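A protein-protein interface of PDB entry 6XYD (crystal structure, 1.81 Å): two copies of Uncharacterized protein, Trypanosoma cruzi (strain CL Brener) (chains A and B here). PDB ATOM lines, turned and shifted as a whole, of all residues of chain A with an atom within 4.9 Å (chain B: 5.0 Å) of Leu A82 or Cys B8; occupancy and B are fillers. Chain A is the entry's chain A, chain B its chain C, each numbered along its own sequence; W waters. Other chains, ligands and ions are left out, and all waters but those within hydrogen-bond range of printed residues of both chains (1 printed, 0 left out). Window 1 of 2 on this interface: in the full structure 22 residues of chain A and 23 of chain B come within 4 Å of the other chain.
OG of Ser A78 lies within hydrogen-bond range of NZ of Lys B112, 2.8 Å away.
OE2 of Glu A86 sits at hydrogen-bond distance from N of Asn B6, at 3.1 Å.
The backbone carbonyl oxygen (O) of Cys B8 lies within hydrogen-bond range of the backbone NH (N) of Leu B21, at 2.9 Å.
OG of Ser B10 lies within hydrogen-bond range of NZ of Lys B112, 2.8 Å away.
The guanidinium group (NH2) of Arg A36 lies within salt-bridge range of the side-chain carboxylate (OE1) of Glu A86, 3.1 Å away.
OG1 of Thr A83 sits close to O of Ala A79, at 3.4 Å.
O of Ser B10 is in hydrogen-bond range of N of Thr B19 (2.8 Å).
Ser A78 touches Ser B10.
Ser A78 touches Leu B21.
Ala A79 touches Leu B21.
CD of Lys B112 touches CE2 of Phe A81, at 3.8 Å.
O of Asn B6 touches CD1 of Leu A82, 3.6 Å away.
Leu A82 touches Cys B8.
C of Leu B21 touches CD2 of Leu A82, at 3.6 Å.
CD2 of Leu A82 touches N of Gly B22, at 3.6 Å.
Ile A85 touches Asn B6 (CG2 to OD1, 3.4 Å).
CD1 of Ile A85 touches CD1 of Phe B114 (3.4 Å).
Of the printed residues of chain B, Ala A79 touches Leu B21.
Printed residues of chain B within 4 Å of Leu A82: Asn B6 (3.6 Å), Leu B7 (3.8 Å), Cys B8 (3.99 Å), Leu B21 (3.6 Å) and Gly B22 (3.6 Å).
Ile A84 touches none of the printed residues of chain B.
Of the printed residues of chain A, Cys B8 touches Leu A82 (3.99 Å).
Val B9 touches none of the printed residues of chain A.
Of the printed residues of chain A, Ser B10 touches Ser A78 (3.9 Å).
Of the 12 printed residues of chain B, 8 touch a printed residue of chain A.
Hydrophobic or aromatic side chains of chain B within 4 Å of the printed part of chain A: Leu B21 and Phe B114.
Of the 11 printed residues of chain A, 6 touch a printed residue of chain B.
Printed residues of chain A that touch a printed residue of chain B: Ser A78, Ala A79, Phe A81, Leu A82, Ile A85 and Glu A86.
No position is printed for both chains.
Of the 14 pairs that touch across the chains among the printed residues, none has its exchanged pair printed and touching as well.
Water W1 lies within hydrogen-bond range of OG of Ser A78 and OG1 of Thr B19.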
ATOM      1  N   ARG A  36       5.179  11.056  16.715  1.00  0.00           N
ATOM      2  CA  ARG A  36       5.141  11.045  18.180  1.00  0.00           C
ATOM      3  C   ARG A  36       4.761   9.684  18.789  1.00  0.00           C
ATOM      4  O   ARG A  36       5.402   9.250  19.744  1.00  0.00           O
ATOM      5  CB  ARG A  36       4.154  12.109  18.694  1.00  0.00           C
ATOM      6  CG  ARG A  36       4.714  13.519  18.760  1.00  0.00           C
ATOM      7  CD  ARG A  36       3.758  14.432  19.517  1.00  0.00           C
ATOM      8  NE  ARG A  36       3.738  14.136  20.952  1.00  0.00           N
ATOM      9  CZ  ARG A  36       4.208  14.954  21.888  1.00  0.00           C
ATOM     10  NH1 ARG A  36       4.679  16.151  21.559  1.00  0.00           N
ATOM     11  NH2 ARG A  36       4.185  14.592  23.164  1.00  0.00           N
ATOM     12  N   SER A  78      -1.210   4.448  28.529  1.00  0.00           N
ATOM     13  CA  SER A  78      -1.137   5.778  29.172  1.00  0.00           C
ATOM     14  C   SER A  78      -0.185   6.672  28.375  1.00  0.00           C
ATOM     15  O   SER A  78      -0.531   7.808  28.080  1.00  0.00           O
ATOM     16  CB  SER A  78      -0.661   5.656  30.619  1.00  0.00           C
ATOM     17  OG  SER A  78      -1.627   4.991  31.411  1.00  0.00           O
ATOM     18  N   ALA A  79       0.996   6.133  27.991  1.00  0.00           N
ATOM     19  CA  ALA A  79       1.994   6.871  27.211  1.00  0.00           C
ATOM     20  C   ALA A  79       1.442   7.276  25.834  1.00  0.00           C
ATOM     21  O   ALA A  79       1.646   8.414  25.417  1.00  0.00           O
ATOM     22  CB  ALA A  79       3.277   6.049  27.066  1.00  0.00           C
ATOM     23  N   VAL A  80       0.672   6.378  25.172  1.00  0.00           N
ATOM     24  CA  VAL A  80       0.045   6.672  23.867  1.00  0.00           C
ATOM     25  C   VAL A  80      -0.965   7.840  24.018  1.00  0.00           C
ATOM     26  O   VAL A  80      -0.913   8.791  23.249  1.00  0.00           O
ATOM     27  CB  VAL A  80      -0.602   5.412  23.234  1.00  0.00           C
ATOM     28  CG1 VAL A  80      -1.569   5.782  22.115  1.00  0.00           C
ATOM     29  CG2 VAL A  80       0.469   4.439  22.731  1.00  0.00           C
ATOM     30  N   PHE A  81      -1.842   7.772  25.035  1.00  0.00           N
ATOM     31  CA  PHE A  81      -2.834   8.840  25.297  1.00  0.00           C
ATOM     32  C   PHE A  81      -2.134  10.163  25.553  1.00  0.00           C
ATOM     33  O   PHE A  81      -2.521  11.183  24.991  1.00  0.00           O
ATOM     34  CB  PHE A  81      -3.729   8.490  26.499  1.00  0.00           C
ATOM     35  CG  PHE A  81      -4.505   7.200  26.378  1.00  0.00           C
ATOM     36  CD1 PHE A  81      -4.929   6.734  25.130  1.00  0.00           C
ATOM     37  CD2 PHE A  81      -4.831   6.454  27.509  1.00  0.00           C
ATOM     38  CE1 PHE A  81      -5.643   5.530  25.022  1.00  0.00           C
ATOM     39  CE2 PHE A  81      -5.550   5.257  27.398  1.00  0.00           C
ATOM     40  CZ  PHE A  81      -5.940   4.801  26.154  1.00  0.00           C
ATOM     41  N   LEU A  82      -1.102  10.141  26.386  1.00  0.00           N
ATOM     42  CA  LEU A  82      -0.369  11.353  26.727  1.00  0.00           C
ATOM     43  C   LEU A  82       0.276  11.992  25.498  1.00  0.00           C
ATOM     44  O   LEU A  82       0.135  13.198  25.312  1.00  0.00           O
ATOM     45  CB  LEU A  82       0.683  11.058  27.804  1.00  0.00           C
ATOM     46  CG  LEU A  82       1.383  12.274  28.400  1.00  0.00           C
ATOM     47  CD1 LEU A  82       0.379  13.270  28.969  1.00  0.00           C
ATOM     48  CD2 LEU A  82       2.338  11.854  29.482  1.00  0.00           C
ATOM     49  N   THR A  83       0.945  11.185  24.637  1.00  0.00           N
ATOM     50  CA  THR A  83       1.611  11.720  23.424  1.00  0.00           C
ATOM     51  C   THR A  83       0.588  12.335  22.483  1.00  0.00           C
ATOM     52  O   THR A  83       0.863  13.373  21.902  1.00  0.00           O
ATOM     53  CB  THR A  83       2.452  10.656  22.687  1.00  0.00           C
ATOM     54  OG1 THR A  83       1.606   9.614  22.206  1.00  0.00           O
ATOM     55  CG2 THR A  83       3.531  10.080  23.532  1.00  0.00           C
ATOM     56  N   ILE A  84      -0.603  11.703  22.354  1.00  0.00           N
ATOM     57  CA  ILE A  84      -1.683  12.214  21.495  1.00  0.00           C
ATOM     58  C   ILE A  84      -2.178  13.552  22.041  1.00  0.00           C
ATOM     59  O   ILE A  84      -2.279  14.515  21.298  1.00  0.00           O
ATOM     60  CB  ILE A  84      -2.828  11.170  21.362  1.00  0.00           C
ATOM     61  CG1 ILE A  84      -2.374   9.955  20.506  1.00  0.00           C
ATOM     62  CG2 ILE A  84      -4.117  11.799  20.793  1.00  0.00           C
ATOM     63  CD1 ILE A  84      -3.345   8.711  20.653  1.00  0.00           C
ATOM     64  N   ILE A  85      -2.482  13.612  23.346  1.00  0.00           N
ATOM     65  CA  ILE A  85      -2.976  14.855  23.957  1.00  0.00           C
ATOM     66  C   ILE A  85      -1.969  15.987  23.803  1.00  0.00           C
ATOM     67  O   ILE A  85      -2.337  17.094  23.400  1.00  0.00           O
ATOM     68  CB  ILE A  85      -3.360  14.605  25.452  1.00  0.00           C
ATOM     69  CG1 ILE A  85      -4.571  13.647  25.535  1.00  0.00           C
ATOM     70  CG2 ILE A  85      -3.644  15.941  26.197  1.00  0.00           C
ATOM     71  CD1 ILE A  85      -4.672  12.867  26.881  1.00  0.00           C
ATOM     72  N   GLU A  86      -0.699  15.719  24.156  1.00  0.00           N
ATOM     73  CA  GLU A  86       0.363  16.742  24.068  1.00  0.00           C
ATOM     74  C   GLU A  86       0.584  17.205  22.643  1.00  0.00           C
ATOM     75  O   GLU A  86       0.685  18.412  22.391  1.00  0.00           O
ATOM     76  CB  GLU A  86       1.670  16.233  24.678  1.00  0.00           C
ATOM     77  CG  GLU A  86       1.599  16.051  26.188  1.00  0.00           C
ATOM     78  CD  GLU A  86       2.905  15.647  26.842  1.00  0.00           C
ATOM     79  OE1 GLU A  86       3.639  14.823  26.252  1.00  0.00           O
ATOM     80  OE2 GLU A  86       3.216  16.188  27.923  1.00  0.00           O
ATOM     81  N   GLY A  87       0.615  16.247  21.708  1.00  0.00           N
ATOM     82  CA  GLY A  87       0.784  16.580  20.295  1.00  0.00           C
ATOM     83  C   GLY A  87      -0.359  17.449  19.797  1.00  0.00           C
ATOM     84  O   GLY A  87      -0.141  18.473  19.152  1.00  0.00           O
ATOM     85  N   ASN B   6       1.420  18.197  29.417  1.00  0.00           N
ATOM     86  CA  ASN B   6       0.271  17.517  30.031  1.00  0.00           C
ATOM     87  C   ASN B   6       0.713  16.374  30.967  1.00  0.00           C
ATOM     88  O   ASN B   6       1.858  15.926  30.891  1.00  0.00           O
ATOM     89  CB  ASN B   6      -0.666  16.948  28.957  1.00  0.00           C
ATOM     90  CG  ASN B   6      -1.447  17.996  28.228  1.00  0.00           C
ATOM     91  OD1 ASN B   6      -2.611  18.258  28.527  1.00  0.00           O
ATOM     92  ND2 ASN B   6      -0.852  18.545  27.198  1.00  0.00           N
ATOM     93  N   LEU B   7      -0.234  15.860  31.793  1.00  0.00           N
ATOM     94  CA  LEU B   7       0.014  14.744  32.670  1.00  0.00           C
ATOM     95  C   LEU B   7      -1.042  13.704  32.477  1.00  0.00           C
ATOM     96  O   LEU B   7      -2.201  14.036  32.233  1.00  0.00           O
ATOM     97  CB  LEU B   7      -0.054  15.158  34.166  1.00  0.00           C
ATOM     98  CG  LEU B   7       0.905  16.172  34.726  1.00  0.00           C
ATOM     99  CD1 LEU B   7       0.702  16.289  36.259  1.00  0.00           C
ATOM    100  CD2 LEU B   7       2.380  15.803  34.419  1.00  0.00           C
ATOM    101  N   CYS B   8      -0.687  12.458  32.722  1.00  0.00           N
ATOM    102  CA  CYS B   8      -1.670  11.376  32.829  1.00  0.00           C
ATOM    103  C   CYS B   8      -1.401  10.642  34.123  1.00  0.00           C
ATOM    104  O   CYS B   8      -0.284  10.147  34.327  1.00  0.00           O
ATOM    105  CB  CYS B   8      -1.636  10.420  31.638  1.00  0.00           C
ATOM    106  SG  CYS B   8      -2.691   8.935  31.864  1.00  0.00           S
ATOM    107  N   VAL B   9      -2.406  10.549  34.989  1.00  0.00           N
ATOM    108  CA  VAL B   9      -2.291   9.770  36.226  1.00  0.00           C
ATOM    109  C   VAL B   9      -3.230   8.579  36.049  1.00  0.00           C
ATOM    110  O   VAL B   9      -4.399   8.764  35.705  1.00  0.00           O
ATOM    111  CB  VAL B   9      -2.627  10.566  37.515  1.00  0.00           C
ATOM    112  CG1 VAL B   9      -2.588   9.662  38.748  1.00  0.00           C
ATOM    113  CG2 VAL B   9      -1.688  11.763  37.691  1.00  0.00           C
ATOM    114  N   SER B  10      -2.712   7.368  36.267  1.00  0.00           N
ATOM    115  CA  SER B  10      -3.505   6.150  36.152  1.00  0.00           C
ATOM    116  C   SER B  10      -3.492   5.406  37.475  1.00  0.00           C
ATOM    117  O   SER B  10      -2.456   5.337  38.141  1.00  0.00           O
ATOM    118  CB  SER B  10      -2.955   5.268  35.034  1.00  0.00           C
ATOM    119  OG  SER B  10      -3.881   4.243  34.715  1.00  0.00           O
ATOM    120  N   THR B  19       0.305   5.296  38.823  1.00  0.00           N
ATOM    121  CA  THR B  19       1.362   5.659  37.872  1.00  0.00           C
ATOM    122  C   THR B  19       1.141   7.084  37.372  1.00  0.00           C
ATOM    123  O   THR B  19       0.001   7.486  37.152  1.00  0.00           O
ATOM    124  CB  THR B  19       1.473   4.630  36.729  1.00  0.00           C
ATOM    125  OG1 THR B  19       0.185   4.434  36.142  1.00  0.00           O
ATOM    126  CG2 THR B  19       2.029   3.283  37.204  1.00  0.00           C
ATOM    127  N   MET B  20       2.216   7.866  37.268  1.00  0.00           N
ATOM    128  CA  MET B  20       2.129   9.257  36.804  1.00  0.00           C
ATOM    129  C   MET B  20       3.091   9.481  35.675  1.00  0.00           C
ATOM    130  O   MET B  20       4.296   9.265  35.842  1.00  0.00           O
ATOM    131  CB  MET B  20       2.385  10.264  37.959  1.00  0.00           C
ATOM    132  CG  MET B  20       1.600   9.942  39.214  1.00  0.00           C
ATOM    133  SD  MET B  20       1.702  11.192  40.514  1.00  0.00           S
ATOM    134  CE  MET B  20       3.407  11.111  40.942  1.00  0.00           C
ATOM    135  N   LEU B  21       2.569   9.921  34.513  1.00  0.00           N
ATOM    136  CA  LEU B  21       3.340  10.171  33.302  1.00  0.00           C
ATOM    137  C   LEU B  21       3.232  11.641  32.946  1.00  0.00           C
ATOM    138  O   LEU B  21       2.164  12.231  33.062  1.00  0.00           O
ATOM    139  CB  LEU B  21       2.772   9.342  32.125  1.00  0.00           C
ATOM    140  CG  LEU B  21       2.934   7.813  32.147  1.00  0.00           C
ATOM    141  CD1 LEU B  21       1.866   7.144  33.022  1.00  0.00           C
ATOM    142  CD2 LEU B  21       2.828   7.274  30.745  1.00  0.00           C
ATOM    143  N   GLY B  22       4.325  12.198  32.462  1.00  0.00           N
ATOM    144  CA  GLY B  22       4.410  13.592  32.080  1.00  0.00           C
ATOM    145  C   GLY B  22       5.789  14.102  32.405  1.00  0.00           C
ATOM    146  O   GLY B  22       6.166  14.150  33.575  1.00  0.00           O
ATOM    147  N   LYS B 112      -8.096   6.663  34.584  1.00  0.00           N
ATOM    148  CA  LYS B 112      -7.108   7.626  34.121  1.00  0.00           C
ATOM    149  C   LYS B 112      -7.598   9.042  34.350  1.00  0.00           C
ATOM    150  O   LYS B 112      -8.782   9.308  34.231  1.00  0.00           O
ATOM    151  CB  LYS B 112      -6.719   7.373  32.677  1.00  0.00           C
ATOM    152  CG  LYS B 112      -6.038   5.989  32.537  1.00  0.00           C
ATOM    153  CD  LYS B 112      -5.608   5.637  31.140  1.00  0.00           C
ATOM    154  CE  LYS B 112      -5.272   4.151  31.079  1.00  0.00           C
ATOM    155  NZ  LYS B 112      -4.111   3.818  31.954  1.00  0.00           N
ATOM    156  N   LEU B 113      -6.681   9.934  34.737  1.00  0.00           N
ATOM    157  CA  LEU B 113      -6.952  11.349  34.979  1.00  0.00           C
ATOM    158  C   LEU B 113      -5.982  12.146  34.143  1.00  0.00           C
ATOM    159  O   LEU B 113      -4.766  11.913  34.225  1.00  0.00           O
ATOM    160  CB  LEU B 113      -6.770  11.700  36.467  1.00  0.00           C
ATOM    161  CG  LEU B 113      -7.704  10.977  37.442  1.00  0.00           C
ATOM    162  CD1 LEU B 113      -7.178  11.109  38.877  1.00  0.00           C
ATOM    163  CD2 LEU B 113      -9.119  11.556  37.358  1.00  0.00           C
ATOM    164  N   PHE B 114      -6.509  13.060  33.304  1.00  0.00           N
ATOM    165  CA  PHE B 114      -5.687  13.836  32.391  1.00  0.00           C
ATOM    166  C   PHE B 114      -5.664  15.298  32.821  1.00  0.00           C
ATOM    167  O   PHE B 114      -6.727  15.895  33.064  1.00  0.00           O
ATOM    168  CB  PHE B 114      -6.199  13.702  30.946  1.00  0.00           C
ATOM    169  CG  PHE B 114      -6.227  12.289  30.419  1.00  0.00           C
ATOM    170  CD1 PHE B 114      -5.059  11.664  30.000  1.00  0.00           C
ATOM    171  CD2 PHE B 114      -7.408  11.552  30.419  1.00  0.00           C
ATOM    172  CE1 PHE B 114      -5.086  10.344  29.507  1.00  0.00           C
ATOM    173  CE2 PHE B 114      -7.426  10.220  29.961  1.00  0.00           C
ATOM    174  CZ  PHE B 114      -6.267   9.641  29.488  1.00  0.00           C
HETATM  175  O   HOH W   1      -0.361   3.615  33.432  1.00  0.00           O
